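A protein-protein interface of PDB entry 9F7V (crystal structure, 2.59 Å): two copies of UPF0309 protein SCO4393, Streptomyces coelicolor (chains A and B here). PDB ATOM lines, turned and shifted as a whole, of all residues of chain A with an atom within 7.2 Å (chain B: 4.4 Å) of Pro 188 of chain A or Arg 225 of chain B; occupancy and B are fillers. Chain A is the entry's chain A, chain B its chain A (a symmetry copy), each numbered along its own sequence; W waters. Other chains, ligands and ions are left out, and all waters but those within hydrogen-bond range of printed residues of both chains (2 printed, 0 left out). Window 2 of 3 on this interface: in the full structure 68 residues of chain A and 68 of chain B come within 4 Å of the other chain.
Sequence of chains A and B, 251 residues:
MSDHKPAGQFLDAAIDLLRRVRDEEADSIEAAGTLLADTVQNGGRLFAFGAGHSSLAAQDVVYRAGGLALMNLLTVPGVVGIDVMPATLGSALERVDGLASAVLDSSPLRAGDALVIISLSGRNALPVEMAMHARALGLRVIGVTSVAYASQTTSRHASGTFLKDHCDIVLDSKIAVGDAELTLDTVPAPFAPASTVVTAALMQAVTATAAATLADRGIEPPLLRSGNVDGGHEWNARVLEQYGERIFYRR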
ATOM      1  N   GLY A 178     -29.279  15.335 -24.255  1.00  0.00           N
ATOM      2  CA  GLY A 178     -27.948  15.296 -24.821  1.00  0.00           C
ATOM      3  C   GLY A 178     -27.582  13.960 -25.428  1.00  0.00           C
ATOM      4  O   GLY A 178     -26.698  13.909 -26.295  1.00  0.00           O
ATOM      5  N   THR A 183     -18.553  11.291 -19.766  1.00  0.00           N
ATOM      6  CA  THR A 183     -17.776  12.516 -19.846  1.00  0.00           C
ATOM      7  C   THR A 183     -16.330  12.224 -19.470  1.00  0.00           C
ATOM      8  O   THR A 183     -16.049  11.300 -18.701  1.00  0.00           O
ATOM      9  CB  THR A 183     -18.376  13.604 -18.940  1.00  0.00           C
ATOM     10  OG1 THR A 183     -17.635  14.821 -19.095  1.00  0.00           O
ATOM     11  CG2 THR A 183     -18.367  13.168 -17.479  1.00  0.00           C
ATOM     12  N   LEU A 184     -15.413  13.012 -20.035  1.00  0.00           N
ATOM     13  CA  LEU A 184     -14.002  12.982 -19.667  1.00  0.00           C
ATOM     14  C   LEU A 184     -13.526  14.395 -19.361  1.00  0.00           C
ATOM     15  O   LEU A 184     -13.849  15.339 -20.089  1.00  0.00           O
ATOM     16  CB  LEU A 184     -13.143  12.366 -20.775  1.00  0.00           C
ATOM     17  CG  LEU A 184     -13.100  10.838 -20.799  1.00  0.00           C
ATOM     18  CD1 LEU A 184     -12.383  10.351 -22.050  1.00  0.00           C
ATOM     19  CD2 LEU A 184     -12.437  10.282 -19.538  1.00  0.00           C
ATOM     20  N   ASP A 185     -12.758  14.533 -18.274  1.00  0.00           N
ATOM     21  CA  ASP A 185     -12.349  15.857 -17.807  1.00  0.00           C
ATOM     22  C   ASP A 185     -11.690  16.684 -18.906  1.00  0.00           C
ATOM     23  O   ASP A 185     -11.955  17.885 -19.029  1.00  0.00           O
ATOM     24  CB  ASP A 185     -11.385  15.717 -16.625  1.00  0.00           C
ATOM     25  CG  ASP A 185     -12.058  15.936 -15.281  1.00  0.00           C
ATOM     26  OD1 ASP A 185     -12.640  17.023 -15.075  1.00  0.00           O
ATOM     27  OD2 ASP A 185     -11.986  15.030 -14.423  1.00  0.00           O
ATOM     28  N   THR A 186     -10.831  16.067 -19.717  1.00  0.00           N
ATOM     29  CA  THR A 186     -10.149  16.810 -20.770  1.00  0.00           C
ATOM     30  C   THR A 186     -11.041  17.125 -21.964  1.00  0.00           C
ATOM     31  O   THR A 186     -10.645  17.935 -22.810  1.00  0.00           O
ATOM     32  CB  THR A 186      -8.920  16.036 -21.262  1.00  0.00           C
ATOM     33  OG1 THR A 186      -8.270  16.779 -22.302  1.00  0.00           O
ATOM     34  CG2 THR A 186      -9.324  14.669 -21.812  1.00  0.00           C
ATOM     35  N   VAL A 187     -12.224  16.532 -22.047  1.00  0.00           N
ATOM     36  CA  VAL A 187     -13.037  16.534 -23.259  1.00  0.00           C
ATOM     37  C   VAL A 187     -14.290  17.360 -22.983  1.00  0.00           C
ATOM     38  O   VAL A 187     -15.065  17.009 -22.083  1.00  0.00           O
ATOM     39  CB  VAL A 187     -13.401  15.108 -23.698  1.00  0.00           C
ATOM     40  CG1 VAL A 187     -14.245  15.141 -24.969  1.00  0.00           C
ATOM     41  CG2 VAL A 187     -12.135  14.284 -23.900  1.00  0.00           C
ATOM     42  N   PRO A 188     -14.541  18.441 -23.728  1.00  0.00           N
ATOM     43  CA  PRO A 188     -15.701  19.285 -23.390  1.00  0.00           C
ATOM     44  C   PRO A 188     -17.044  18.648 -23.705  1.00  0.00           C
ATOM     45  O   PRO A 188     -18.001  18.841 -22.943  1.00  0.00           O
ATOM     46  CB  PRO A 188     -15.460  20.552 -24.224  1.00  0.00           C
ATOM     47  CG  PRO A 188     -14.614  20.103 -25.367  1.00  0.00           C
ATOM     48  CD  PRO A 188     -13.737  19.012 -24.824  1.00  0.00           C
ATOM     49  N   ALA A 189     -17.154  17.892 -24.800  1.00  0.00           N
ATOM     50  CA  ALA A 189     -18.468  17.331 -25.104  1.00  0.00           C
ATOM     51  C   ALA A 189     -18.641  15.949 -24.474  1.00  0.00           C
ATOM     52  O   ALA A 189     -17.680  15.180 -24.389  1.00  0.00           O
ATOM     53  CB  ALA A 189     -18.670  17.220 -26.612  1.00  0.00           C
ATOM     54  N   PRO A 190     -19.847  15.621 -24.018  1.00  0.00           N
ATOM     55  CA  PRO A 190     -20.136  14.242 -23.618  1.00  0.00           C
ATOM     56  C   PRO A 190     -20.172  13.323 -24.829  1.00  0.00           C
ATOM     57  O   PRO A 190     -20.339  13.760 -25.968  1.00  0.00           O
ATOM     58  CB  PRO A 190     -21.509  14.356 -22.953  1.00  0.00           C
ATOM     59  CG  PRO A 190     -22.170  15.421 -23.745  1.00  0.00           C
ATOM     60  CD  PRO A 190     -21.071  16.443 -23.990  1.00  0.00           C
ATOM     61  N   ALA B  65     -24.994  11.862 -32.251  1.00  0.00           N
ATOM     62  CA  ALA B  65     -24.811  12.563 -30.984  1.00  0.00           C
ATOM     63  C   ALA B  65     -23.895  11.768 -30.067  1.00  0.00           C
ATOM     64  O   ALA B  65     -24.161  10.603 -29.760  1.00  0.00           O
ATOM     65  CB  ALA B  65     -26.165  12.795 -30.310  1.00  0.00           C
ATOM     66  N   LEU B 223     -15.785  14.949 -31.604  1.00  0.00           N
ATOM     67  CA  LEU B 223     -17.092  14.470 -31.182  1.00  0.00           C
ATOM     68  C   LEU B 223     -18.195  15.403 -31.661  1.00  0.00           C
ATOM     69  O   LEU B 223     -18.034  16.629 -31.666  1.00  0.00           O
ATOM     70  CB  LEU B 223     -17.152  14.341 -29.659  1.00  0.00           C
ATOM     71  CG  LEU B 223     -16.320  13.209 -29.057  1.00  0.00           C
ATOM     72  CD1 LEU B 223     -16.180  13.414 -27.557  1.00  0.00           C
ATOM     73  CD2 LEU B 223     -16.936  11.850 -29.371  1.00  0.00           C
ATOM     74  N   LEU B 224     -19.324  14.810 -32.042  1.00  0.00           N
ATOM     75  CA  LEU B 224     -20.529  15.532 -32.419  1.00  0.00           C
ATOM     76  C   LEU B 224     -21.478  15.651 -31.234  1.00  0.00           C
ATOM     77  O   LEU B 224     -21.448  14.840 -30.305  1.00  0.00           O
ATOM     78  CB  LEU B 224     -21.240  14.832 -33.581  1.00  0.00           C
ATOM     79  CG  LEU B 224     -20.409  14.635 -34.847  1.00  0.00           C
ATOM     80  CD1 LEU B 224     -21.154  13.769 -35.847  1.00  0.00           C
ATOM     81  CD2 LEU B 224     -20.060  15.977 -35.460  1.00  0.00           C
ATOM     82  N   ARG B 225     -22.308  16.688 -31.267  1.00  0.00           N
ATOM     83  CA  ARG B 225     -23.371  16.892 -30.295  1.00  0.00           C
ATOM     84  C   ARG B 225     -24.725  16.590 -30.926  1.00  0.00           C
ATOM     85  O   ARG B 225     -24.871  16.564 -32.151  1.00  0.00           O
ATOM     86  CB  ARG B 225     -23.353  18.334 -29.779  1.00  0.00           C
ATOM     87  CG  ARG B 225     -22.196  18.630 -28.849  1.00  0.00           C
ATOM     88  CD  ARG B 225     -22.275  20.041 -28.298  1.00  0.00           C
ATOM     89  NE  ARG B 225     -21.254  20.277 -27.285  1.00  0.00           N
ATOM     90  CZ  ARG B 225     -21.415  20.046 -25.990  1.00  0.00           C
ATOM     91  NH1 ARG B 225     -22.525  19.498 -25.517  1.00  0.00           N
ATOM     92  NH2 ARG B 225     -20.430  20.351 -25.149  1.00  0.00           N
ATOM     93  N   SER B 226     -25.727  16.373 -30.078  1.00  0.00           N
ATOM     94  CA  SER B 226     -27.068  16.118 -30.589  1.00  0.00           C
ATOM     95  C   SER B 226     -27.596  17.371 -31.275  1.00  0.00           C
ATOM     96  O   SER B 226     -27.560  18.465 -30.705  1.00  0.00           O
ATOM     97  CB  SER B 226     -27.997  15.703 -29.448  1.00  0.00           C
ATOM     98  OG  SER B 226     -29.325  15.506 -29.908  1.00  0.00           O
ATOM     99  N   GLY B 227     -28.136  17.203 -32.483  1.00  0.00           N
ATOM    100  CA  GLY B 227     -28.820  18.300 -33.143  1.00  0.00           C
ATOM    101  C   GLY B 227     -30.169  18.666 -32.572  1.00  0.00           C
ATOM    102  O   GLY B 227     -30.767  19.643 -33.031  1.00  0.00           O
ATOM    103  N   GLY B 232     -26.632  22.333 -31.177  1.00  0.00           N
ATOM    104  CA  GLY B 232     -25.925  21.148 -31.630  1.00  0.00           C
ATOM    105  C   GLY B 232     -25.497  21.245 -33.081  1.00  0.00           C
ATOM    106  O   GLY B 232     -24.378  20.863 -33.435  1.00  0.00           O
ATOM    107  N   TRP B 235     -22.508  23.554 -33.455  1.00  0.00           N
ATOM    108  CA  TRP B 235     -21.319  22.825 -33.030  1.00  0.00           C
ATOM    109  C   TRP B 235     -20.856  21.856 -34.114  1.00  0.00           C
ATOM    110  O   TRP B 235     -19.681  21.845 -34.494  1.00  0.00           O
ATOM    111  CB  TRP B 235     -21.614  22.093 -31.720  1.00  0.00           C
ATOM    112  CG  TRP B 235     -20.514  21.202 -31.223  1.00  0.00           C
ATOM    113  CD1 TRP B 235     -20.203  19.947 -31.667  1.00  0.00           C
ATOM    114  CD2 TRP B 235     -19.587  21.497 -30.174  1.00  0.00           C
ATOM    115  NE1 TRP B 235     -19.135  19.447 -30.959  1.00  0.00           N
ATOM    116  CE2 TRP B 235     -18.738  20.380 -30.039  1.00  0.00           C
ATOM    117  CE3 TRP B 235     -19.389  22.600 -29.336  1.00  0.00           C
ATOM    118  CZ2 TRP B 235     -17.710  20.334 -29.101  1.00  0.00           C
ATOM    119  CZ3 TRP B 235     -18.367  22.551 -28.408  1.00  0.00           C
ATOM    120  CH2 TRP B 235     -17.540  21.428 -28.297  1.00  0.00           C
ATOM    121  N   ASN B 236     -21.780  21.042 -34.638  1.00  0.00           N
ATOM    122  CA  ASN B 236     -21.396  20.013 -35.600  1.00  0.00           C
ATOM    123  C   ASN B 236     -20.869  20.620 -36.892  1.00  0.00           C
ATOM    124  O   ASN B 236     -19.934  20.081 -37.497  1.00  0.00           O
ATOM    125  CB  ASN B 236     -22.580  19.096 -35.909  1.00  0.00           C
ATOM    126  CG  ASN B 236     -23.006  18.261 -34.722  1.00  0.00           C
ATOM    127  OD1 ASN B 236     -22.314  18.192 -33.708  1.00  0.00           O
ATOM    128  ND2 ASN B 236     -24.150  17.604 -34.853  1.00  0.00           N
HETATM  129  O   HOH W   1     -24.748  15.370 -27.281  1.00  0.00           O
HETATM  130  O   HOH W   2     -22.024  15.287 -27.508  1.00  0.00           O
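The backbone carbonyl oxygen (O) of Leu 223 of chain B is in hydrogen-bond range of the indole nitrogen (NE1) of Trp 235 of chain B.
The side-chain amide oxygen (OD1) of Asn 236 of chain B lies within hydrogen-bond range of the backbone NH (N) of Arg 225 of chain B.
Ser 226 of chain B touches Gly 178 of chain A (CB to O, 3.9 Å).
CD1 of Leu 223 of chain B touches CG1 of Val 187 of chain A, at 3.7 Å.
O of Pro 188 of chain A touches NH2 of Arg 225 of chain B, 3.6 Å away.
Ala 189 of chain A touches Leu 223 of chain B (O to CD1, 3.9 Å).
CA of Ala 189 of chain A touches NH2 of Arg 225 of chain B (3.6 Å).
Arg 225 of chain B touches Pro 190 of chain A (NH1 to CD, 3.7 Å).
Of chain B, only Arg 225 comes within 4 Å of Pro 188 of chain A.
Arg 225 of chain B touches just these residues of chain A: Pro 188, Ala 189 and Pro 190.
Of the printed residues of chain A, Ser 226 of chain B touches Gly 178 (3.9 Å).
Of the printed residues of chain A, Leu 223 of chain B touches Val 187 (3.7 Å) and Ala 189 (3.9 Å).
Gly 227 of chain B touches none of the printed residues of chain A.
Thr 183 of chain A touches none of the printed residues of chain B.
The nearest residue of chain B that does not touch Pro 188 of chain A is Trp 235 of chain B (4.3 Å).
The nearest residue of chain A that does not touch Arg 225 of chain B is Gly 178 of chain A (5.7 Å).
Printed residues of chain B that touch a printed residue of chain A: Leu 223, Arg 225 and Ser 226.
Printed residues of chain A that touch a printed residue of chain B: Gly 178, Val 187, Pro 188, Ala 189 and Pro 190.
Hydrophobic or aromatic side chains of chain A within 4 Å of the printed part of chain B: Val 187, Ala 189 and Pro 190.
No position is printed for both chains.
Of the 6 pairs that touch across the chains among the printed residues, none has its exchanged pair printed and touching as well.
Water W1 bridges O of Gly 178 of chain A (2.6 Å) and N of Ser 226 of chain B (3.1 Å).
Water W2 bridges the backbone carbonyl oxygen (O) of Pro 190 of chain A and the backbone carbonyl oxygen (O) of Leu 224 of chain B.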
